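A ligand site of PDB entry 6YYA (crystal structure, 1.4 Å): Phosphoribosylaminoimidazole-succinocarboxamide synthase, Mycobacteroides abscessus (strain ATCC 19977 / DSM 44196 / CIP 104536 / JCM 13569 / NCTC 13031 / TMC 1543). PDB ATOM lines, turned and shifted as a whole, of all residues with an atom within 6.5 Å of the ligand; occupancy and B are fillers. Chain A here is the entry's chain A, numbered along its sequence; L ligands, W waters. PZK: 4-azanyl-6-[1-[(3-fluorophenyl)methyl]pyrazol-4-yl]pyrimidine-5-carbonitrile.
N of Arg 100 is in hydrogen-bond range of O of His 78.
A ring nitrogen (NE2) of His 78 is in hydrogen-bond range of the backbone carbonyl oxygen of Asp 222 (3.4 Å).
The backbone NH (N) of Leu 28 is in hydrogen-bond range of the backbone carbonyl oxygen (O) of Ala 21.
OG of Ser 22 lies within hydrogen-bond range of NE2 of His 19 (2.6 Å).
The backbone NH (N) of Val 20 sits at hydrogen-bond distance from the backbone carbonyl oxygen (O) of Leu 28 (2.9 Å).
The guanidinium group (NH1) of Arg 26 is in salt-bridge range of the side-chain carboxylate (OD1) of Asp 222, at 2.7 Å.
The side-chain carboxylate (OE2) of Glu 223 lies within salt-bridge range of the guanidinium group (NH1) of Arg 26, at 3.3 Å.
The backbone NH (N) of Glu 209 sits at hydrogen-bond distance from the side-chain carboxylate (OD2) of Asp 222, at 3.0 Å.
O of Ala 21 sits close to F22 of the ligand (3.2 Å).
N of Ser 22 lies close to F22 of the ligand, 3.4 Å away.
N of Gly 23 sits close to F22 of the ligand (3.2 Å).
The backbone carbonyl oxygen (O) of Arg 26 sits close to a fluorine (F22) of the ligand, at 3.5 Å.
Glu 27 touches the ligand.
Leu 28 touches the ligand.
Leu 36 touches the ligand (CD1 to N03, 3.7 Å).
CE2 of Phe 38 touches C18 of the ligand, 3.3 Å away.
CG2 of Val 99 touches N01 of the ligand, at 3.97 Å.
CA of Arg 101 touches N03 of the ligand, at 3.6 Å.
Met 104 touches the ligand (CG to N05, 3.3 Å).
Glu 209 touches the ligand.
Ala 221 touches the ligand.
Hydrophobic or aromatic side chains within 4 Å of the ligand: Ala 21, Leu 28, Leu 36, Phe 38, His 78, Val 99, Leu 102 and Met 104.
The nearest printed residue that does not touch the ligand is Asp 222 (4.5 Å).
A nitrogen (N01) of the ligand sits at hydrogen-bond distance from the backbone carbonyl oxygen of Arg 100, at 2.9 Å.
N03 of the ligand sits at hydrogen-bond distance from N of Leu 102, at 2.9 Å.
A ring nitrogen (ND1) of His 78 sits at hydrogen-bond distance from a nitrogen (N01) of the ligand (3.0 Å).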
ATOM      1  N   HIS A  19       9.375 -12.406   6.855  1.00  0.00           N
ATOM      2  CA  HIS A  19       8.638 -13.636   6.612  1.00  0.00           C
ATOM      3  C   HIS A  19       8.377 -14.355   7.934  1.00  0.00           C
ATOM      4  O   HIS A  19       9.292 -14.592   8.717  1.00  0.00           O
ATOM      5  CB  HIS A  19       9.400 -14.567   5.650  1.00  0.00           C
ATOM      6  CG  HIS A  19       8.796 -15.931   5.496  1.00  0.00           C
ATOM      7  ND1 HIS A  19       9.391 -17.073   6.002  1.00  0.00           N
ATOM      8  CD2 HIS A  19       7.666 -16.335   4.885  1.00  0.00           C
ATOM      9  CE1 HIS A  19       8.641 -18.117   5.707  1.00  0.00           C
ATOM     10  NE2 HIS A  19       7.577 -17.701   5.036  1.00  0.00           N
ATOM     11  N   VAL A  20       7.106 -14.656   8.188  1.00  0.00           N
ATOM     12  CA  VAL A  20       6.771 -15.306   9.452  1.00  0.00           C
ATOM     13  C   VAL A  20       6.087 -16.662   9.286  1.00  0.00           C
ATOM     14  O   VAL A  20       6.066 -17.453  10.227  1.00  0.00           O
ATOM     15  CB  VAL A  20       5.875 -14.384  10.324  1.00  0.00           C
ATOM     16  CG1 VAL A  20       6.623 -13.105  10.671  1.00  0.00           C
ATOM     17  CG2 VAL A  20       4.552 -14.058   9.608  1.00  0.00           C
ATOM     18  N   ALA A  21       5.534 -16.936   8.101  1.00  0.00           N
ATOM     19  CA  ALA A  21       4.926 -18.241   7.866  1.00  0.00           C
ATOM     20  C   ALA A  21       4.818 -18.571   6.386  1.00  0.00           C
ATOM     21  O   ALA A  21       4.654 -17.692   5.541  1.00  0.00           O
ATOM     22  CB  ALA A  21       3.535 -18.299   8.505  1.00  0.00           C
ATOM     23  N   SER A  22       4.915 -19.863   6.085  1.00  0.00           N
ATOM     24  CA  SER A  22       4.714 -20.384   4.740  1.00  0.00           C
ATOM     25  C   SER A  22       3.775 -21.585   4.763  1.00  0.00           C
ATOM     26  O   SER A  22       3.919 -22.484   5.599  1.00  0.00           O
ATOM     27  CB  SER A  22       6.031 -20.802   4.090  1.00  0.00           C
ATOM     28  OG  SER A  22       6.742 -19.676   3.607  1.00  0.00           O
ATOM     29  N   GLY A  23       2.807 -21.591   3.852  1.00  0.00           N
ATOM     30  CA  GLY A  23       1.958 -22.741   3.631  1.00  0.00           C
ATOM     31  C   GLY A  23       2.246 -23.279   2.241  1.00  0.00           C
ATOM     32  O   GLY A  23       3.162 -22.803   1.559  1.00  0.00           O
ATOM     33  N   LYS A  24       1.452 -24.257   1.820  1.00  0.00           N
ATOM     34  CA  LYS A  24       1.649 -24.895   0.526  1.00  0.00           C
ATOM     35  C   LYS A  24       1.628 -23.904  -0.636  1.00  0.00           C
ATOM     36  O   LYS A  24       2.453 -23.970  -1.538  1.00  0.00           O
ATOM     37  CB  LYS A  24       0.573 -25.970   0.307  1.00  0.00           C
ATOM     38  N   ARG A  26       0.600 -20.317  -0.002  1.00  0.00           N
ATOM     39  CA  ARG A  26       0.479 -18.955   0.528  1.00  0.00           C
ATOM     40  C   ARG A  26       1.620 -18.618   1.480  1.00  0.00           C
ATOM     41  O   ARG A  26       2.327 -19.501   1.966  1.00  0.00           O
ATOM     42  CB  ARG A  26      -0.884 -18.788   1.228  1.00  0.00           C
ATOM     43  CG  ARG A  26      -1.082 -19.754   2.344  1.00  0.00           C
ATOM     44  CD  ARG A  26      -2.535 -19.777   2.764  1.00  0.00           C
ATOM     45  NE  ARG A  26      -2.690 -20.431   4.061  1.00  0.00           N
ATOM     46  CZ  ARG A  26      -3.825 -20.430   4.746  1.00  0.00           C
ATOM     47  NH1 ARG A  26      -4.894 -19.807   4.252  1.00  0.00           N
ATOM     48  NH2 ARG A  26      -3.887 -21.039   5.920  1.00  0.00           N
ATOM     49  N   GLU A  27       1.812 -17.329   1.745  1.00  0.00           N
ATOM     50  CA  GLU A  27       2.911 -16.855   2.578  1.00  0.00           C
ATOM     51  C   GLU A  27       2.412 -15.735   3.470  1.00  0.00           C
ATOM     52  O   GLU A  27       1.443 -15.058   3.131  1.00  0.00           O
ATOM     53  CB  GLU A  27       4.074 -16.360   1.709  1.00  0.00           C
ATOM     54  CG  GLU A  27       4.763 -17.415   0.864  1.00  0.00           C
ATOM     55  CD  GLU A  27       5.690 -16.799  -0.160  1.00  0.00           C
ATOM     56  OE1 GLU A  27       5.555 -15.587  -0.426  1.00  0.00           O
ATOM     57  OE2 GLU A  27       6.560 -17.533  -0.689  1.00  0.00           O
ATOM     58  N   LEU A  28       3.066 -15.534   4.599  1.00  0.00           N
ATOM     59  CA  LEU A  28       2.652 -14.507   5.563  1.00  0.00           C
ATOM     60  C   LEU A  28       3.853 -13.687   5.990  1.00  0.00           C
ATOM     61  O   LEU A  28       4.898 -14.250   6.347  1.00  0.00           O
ATOM     62  CB  LEU A  28       1.963 -15.158   6.767  1.00  0.00           C
ATOM     63  CG  LEU A  28       1.217 -14.235   7.727  1.00  0.00           C
ATOM     64  CD1 LEU A  28       0.047 -13.534   7.035  1.00  0.00           C
ATOM     65  CD2 LEU A  28       0.738 -15.030   8.907  1.00  0.00           C
ATOM     66  N   LEU A  36      -0.069  -7.619   9.198  1.00  0.00           N
ATOM     67  CA  LEU A  36       0.603  -8.610   8.383  1.00  0.00           C
ATOM     68  C   LEU A  36       0.238  -8.412   6.942  1.00  0.00           C
ATOM     69  O   LEU A  36      -0.739  -7.734   6.597  1.00  0.00           O
ATOM     70  CB  LEU A  36       0.206 -10.023   8.824  1.00  0.00           C
ATOM     71  CG  LEU A  36       0.297 -10.303  10.317  1.00  0.00           C
ATOM     72  CD1 LEU A  36      -0.267 -11.692  10.648  1.00  0.00           C
ATOM     73  CD2 LEU A  36       1.707 -10.177  10.833  1.00  0.00           C
ATOM     74  N   LEU A  37       1.017  -9.055   6.078  1.00  0.00           N
ATOM     75  CA  LEU A  37       0.763  -9.120   4.656  1.00  0.00           C
ATOM     76  C   LEU A  37       0.490 -10.565   4.277  1.00  0.00           C
ATOM     77  O   LEU A  37       1.341 -11.437   4.446  1.00  0.00           O
ATOM     78  CB  LEU A  37       1.956  -8.564   3.884  1.00  0.00           C
ATOM     79  CG  LEU A  37       1.731  -8.456   2.387  1.00  0.00           C
ATOM     80  CD1 LEU A  37       0.859  -7.259   2.052  1.00  0.00           C
ATOM     81  CD2 LEU A  37       3.078  -8.392   1.660  1.00  0.00           C
ATOM     82  N   PHE A  38      -0.727 -10.821   3.808  1.00  0.00           N
ATOM     83  CA  PHE A  38      -1.213 -12.155   3.468  1.00  0.00           C
ATOM     84  C   PHE A  38      -1.029 -12.347   1.968  1.00  0.00           C
ATOM     85  O   PHE A  38      -1.676 -11.662   1.192  1.00  0.00           O
ATOM     86  CB  PHE A  38      -2.689 -12.268   3.870  1.00  0.00           C
ATOM     87  CG  PHE A  38      -3.242 -13.674   3.869  1.00  0.00           C
ATOM     88  CD1 PHE A  38      -3.386 -14.380   2.681  1.00  0.00           C
ATOM     89  CD2 PHE A  38      -3.705 -14.241   5.048  1.00  0.00           C
ATOM     90  CE1 PHE A  38      -3.913 -15.665   2.697  1.00  0.00           C
ATOM     91  CE2 PHE A  38      -4.255 -15.506   5.063  1.00  0.00           C
ATOM     92  CZ  PHE A  38      -4.355 -16.222   3.883  1.00  0.00           C
ATOM     93  N   VAL A  39      -0.153 -13.273   1.562  1.00  0.00           N
ATOM     94  CA  VAL A  39       0.197 -13.402   0.155  1.00  0.00           C
ATOM     95  C   VAL A  39      -0.233 -14.732  -0.460  1.00  0.00           C
ATOM     96  O   VAL A  39       0.129 -15.790   0.058  1.00  0.00           O
ATOM     97  CB  VAL A  39       1.712 -13.232  -0.036  1.00  0.00           C
ATOM     98  CG1 VAL A  39       2.068 -13.398  -1.503  1.00  0.00           C
ATOM     99  CG2 VAL A  39       2.174 -11.868   0.481  1.00  0.00           C
ATOM    100  N   HIS A  78     -10.425  -9.748   9.126  1.00  0.00           N
ATOM    101  CA  HIS A  78      -9.067  -9.215   9.417  1.00  0.00           C
ATOM    102  C   HIS A  78      -8.531  -8.230   8.367  1.00  0.00           C
ATOM    103  O   HIS A  78      -7.474  -7.760   8.571  1.00  0.00           O
ATOM    104  CB  HIS A  78      -8.093 -10.364   9.666  1.00  0.00           C
ATOM    105  CG  HIS A  78      -7.717 -11.165   8.464  1.00  0.00           C
ATOM    106  ND1 HIS A  78      -6.632 -11.957   8.439  1.00  0.00           N
ATOM    107  CD2 HIS A  78      -8.322 -11.330   7.279  1.00  0.00           C
ATOM    108  CE1 HIS A  78      -6.550 -12.541   7.277  1.00  0.00           C
ATOM    109  NE2 HIS A  78      -7.564 -12.180   6.553  1.00  0.00           N
ATOM    110  N   VAL A  99      -3.508  -7.094   6.499  1.00  0.00           N
ATOM    111  CA  VAL A  99      -4.447  -7.600   7.489  1.00  0.00           C
ATOM    112  C   VAL A  99      -4.031  -7.267   8.911  1.00  0.00           C
ATOM    113  O   VAL A  99      -2.858  -6.999   9.183  1.00  0.00           O
ATOM    114  CB  VAL A  99      -4.585  -9.093   7.320  1.00  0.00           C
ATOM    115  CG1 VAL A  99      -4.987  -9.378   5.871  1.00  0.00           C
ATOM    116  CG2 VAL A  99      -3.314  -9.868   7.688  1.00  0.00           C
ATOM    117  N   ARG A 100      -5.001  -7.244   9.825  1.00  0.00           N
ATOM    118  CA  ARG A 100      -4.725  -6.955  11.222  1.00  0.00           C
ATOM    119  C   ARG A 100      -4.233  -8.209  11.917  1.00  0.00           C
ATOM    120  O   ARG A 100      -4.803  -9.289  11.698  1.00  0.00           O
ATOM    121  CB  ARG A 100      -5.965  -6.450  11.963  1.00  0.00           C
ATOM    122  CG  ARG A 100      -6.848  -5.449  11.265  1.00  0.00           C
ATOM    123  CD  ARG A 100      -8.059  -5.122  12.168  1.00  0.00           C
ATOM    124  NE  ARG A 100      -9.239  -5.947  11.905  1.00  0.00           N
ATOM    125  CZ  ARG A 100     -10.117  -6.304  12.843  1.00  0.00           C
ATOM    126  NH1 ARG A 100      -9.944  -5.941  14.106  1.00  0.00           N
ATOM    127  NH2 ARG A 100     -11.173  -7.045  12.521  1.00  0.00           N
ATOM    128  N   ARG A 101      -3.231  -8.076  12.772  1.00  0.00           N
ATOM    129  CA  ARG A 101      -2.737  -9.196  13.561  1.00  0.00           C
ATOM    130  C   ARG A 101      -3.751  -9.575  14.646  1.00  0.00           C
ATOM    131  O   ARG A 101      -4.223  -8.721  15.403  1.00  0.00           O
ATOM    132  CB  ARG A 101      -1.398  -8.869  14.208  1.00  0.00           C
ATOM    133  CG  ARG A 101      -0.702 -10.072  14.836  1.00  0.00           C
ATOM    134  CD  ARG A 101       0.534  -9.663  15.635  1.00  0.00           C
ATOM    135  NE  ARG A 101       0.203  -8.740  16.721  1.00  0.00           N
ATOM    136  CZ  ARG A 101      -0.290  -9.134  17.897  1.00  0.00           C
ATOM    137  NH1 ARG A 101      -0.521 -10.418  18.139  1.00  0.00           N
ATOM    138  NH2 ARG A 101      -0.558  -8.236  18.840  1.00  0.00           N
ATOM    139  N   LEU A 102      -4.074 -10.867  14.713  1.00  0.00           N
ATOM    140  CA  LEU A 102      -4.997 -11.385  15.714  1.00  0.00           C
ATOM    141  C   LEU A 102      -4.357 -12.495  16.550  1.00  0.00           C
ATOM    142  O   LEU A 102      -3.341 -13.073  16.149  1.00  0.00           O
ATOM    143  CB  LEU A 102      -6.253 -11.938  15.046  1.00  0.00           C
ATOM    144  CG  LEU A 102      -7.086 -11.016  14.166  1.00  0.00           C
ATOM    145  CD1 LEU A 102      -7.943 -11.870  13.269  1.00  0.00           C
ATOM    146  CD2 LEU A 102      -7.936 -10.083  14.999  1.00  0.00           C
ATOM    147  N   ASP A 103      -4.966 -12.817  17.687  1.00  0.00           N
ATOM    148  CA  ASP A 103      -4.617 -14.044  18.402  1.00  0.00           C
ATOM    149  C   ASP A 103      -5.435 -15.173  17.782  1.00  0.00           C
ATOM    150  O   ASP A 103      -6.638 -15.259  17.968  1.00  0.00           O
ATOM    151  CB  ASP A 103      -4.891 -13.907  19.891  1.00  0.00           C
ATOM    152  CG  ASP A 103      -3.915 -12.970  20.591  1.00  0.00           C
ATOM    153  OD1 ASP A 103      -2.799 -12.769  20.054  1.00  0.00           O
ATOM    154  OD2 ASP A 103      -4.270 -12.434  21.653  1.00  0.00           O
ATOM    155  N   MET A 104      -4.774 -16.019  17.001  1.00  0.00           N
ATOM    156  CA  MET A 104      -5.468 -17.057  16.244  1.00  0.00           C
ATOM    157  C   MET A 104      -5.961 -18.189  17.141  1.00  0.00           C
ATOM    158  O   MET A 104      -5.274 -18.617  18.063  1.00  0.00           O
ATOM    159  CB  MET A 104      -4.552 -17.597  15.148  1.00  0.00           C
ATOM    160  CG  MET A 104      -4.176 -16.522  14.148  1.00  0.00           C
ATOM    161  SD  MET A 104      -5.596 -15.839  13.237  1.00  0.00           S
ATOM    162  CE  MET A 104      -6.142 -17.301  12.350  1.00  0.00           C
ATOM    163  N   GLU A 209     -10.206 -20.233   9.337  1.00  0.00           N
ATOM    164  CA  GLU A 209      -9.641 -19.980  10.662  1.00  0.00           C
ATOM    165  C   GLU A 209     -10.124 -18.632  11.187  1.00  0.00           C
ATOM    166  O   GLU A 209     -10.338 -17.674  10.429  1.00  0.00           O
ATOM    167  CB  GLU A 209      -8.110 -19.999  10.632  1.00  0.00           C
ATOM    168  CG  GLU A 209      -7.506 -21.349  10.291  1.00  0.00           C
ATOM    169  CD  GLU A 209      -5.982 -21.297  10.169  1.00  0.00           C
ATOM    170  OE1 GLU A 209      -5.419 -20.183  10.148  1.00  0.00           O
ATOM    171  OE2 GLU A 209      -5.360 -22.374  10.082  1.00  0.00           O
ATOM    172  N   ALA A 221     -10.406 -14.774   9.721  1.00  0.00           N
ATOM    173  CA  ALA A 221      -8.992 -14.476   9.481  1.00  0.00           C
ATOM    174  C   ALA A 221      -8.318 -15.513   8.642  1.00  0.00           C
ATOM    175  O   ALA A 221      -7.474 -16.255   9.139  1.00  0.00           O
ATOM    176  CB  ALA A 221      -8.241 -14.319  10.788  1.00  0.00           C
ATOM    177  N   ASP A 222      -8.684 -15.550   7.376  1.00  0.00           N
ATOM    178  CA  ASP A 222      -8.130 -16.555   6.497  1.00  0.00           C
ATOM    179  C   ASP A 222      -8.355 -16.066   5.085  1.00  0.00           C
ATOM    180  O   ASP A 222      -8.709 -14.908   4.857  1.00  0.00           O
ATOM    181  CB  ASP A 222      -8.834 -17.892   6.737  1.00  0.00           C
ATOM    182  CG  ASP A 222      -7.947 -19.091   6.452  1.00  0.00           C
ATOM    183  OD1 ASP A 222      -7.216 -19.084   5.423  1.00  0.00           O
ATOM    184  OD2 ASP A 222      -8.007 -20.056   7.242  1.00  0.00           O
ATOM    185  N   GLU A 223      -8.146 -16.943   4.122  1.00  0.00           N
ATOM    186  CA  GLU A 223      -8.778 -16.726   2.835  1.00  0.00           C
ATOM    187  C   GLU A 223     -10.143 -17.349   2.984  1.00  0.00           C
ATOM    188  O   GLU A 223     -10.319 -18.324   3.739  1.00  0.00           O
ATOM    189  CB  GLU A 223      -7.972 -17.348   1.703  1.00  0.00           C
ATOM    190  CG  GLU A 223      -7.832 -18.843   1.812  1.00  0.00           C
ATOM    191  CD  GLU A 223      -6.805 -19.386   0.851  1.00  0.00           C
ATOM    192  OE1 GLU A 223      -7.196 -20.031  -0.140  1.00  0.00           O
ATOM    193  OE2 GLU A 223      -5.599 -19.137   1.079  1.00  0.00           O
HETATM  194  C10 PZK L   1      -2.005 -16.265  10.786  1.00  0.00           C
HETATM  195  N12 PZK L   1      -1.829 -18.092   9.604  1.00  0.00           N
HETATM  196  C15 PZK L   1      -2.058 -19.127   8.613  1.00  0.00           C
HETATM  197  C17 PZK L   1      -2.042 -17.742   6.545  1.00  0.00           C
HETATM  198  C20 PZK L   1       0.486 -18.551   5.729  1.00  0.00           C
HETATM  199  C21 PZK L   1      -0.066 -19.057   6.929  1.00  0.00           C
HETATM  200  N01 PZK L   1      -4.682 -11.986  10.759  1.00  0.00           N
HETATM  201  C02 PZK L   1      -3.767 -12.872  11.369  1.00  0.00           C
HETATM  202  N03 PZK L   1      -3.242 -12.594  12.572  1.00  0.00           N
HETATM  203  C04 PZK L   1      -2.375 -13.443  13.138  1.00  0.00           C
HETATM  204  N05 PZK L   1      -2.008 -14.571  12.563  1.00  0.00           N
HETATM  205  C06 PZK L   1      -2.473 -14.943  11.384  1.00  0.00           C
HETATM  206  C07 PZK L   1      -3.400 -14.057  10.724  1.00  0.00           C
HETATM  207  C08 PZK L   1      -3.996 -14.370   9.382  1.00  0.00           C
HETATM  208  N09 PZK L   1      -4.455 -14.585   8.376  1.00  0.00           N
HETATM  209  C11 PZK L   1      -2.587 -16.996   9.795  1.00  0.00           C
HETATM  210  N13 PZK L   1      -0.782 -18.077  10.451  1.00  0.00           N
HETATM  211  C14 PZK L   1      -0.863 -16.970  11.211  1.00  0.00           C
HETATM  212  C16 PZK L   1      -1.362 -18.630   7.317  1.00  0.00           C
HETATM  213  C18 PZK L   1      -1.487 -17.232   5.374  1.00  0.00           C
HETATM  214  C19 PZK L   1      -0.186 -17.654   4.966  1.00  0.00           C
HETATM  215  F22 PZK L   1       1.735 -18.947   5.324  1.00  0.00           F
HETATM  216  O   HOH W   1      -0.678 -16.201  14.540  1.00  0.00           O
HETATM  217  O   HOH W   2      -5.349 -17.945   8.182  1.00  0.00           O
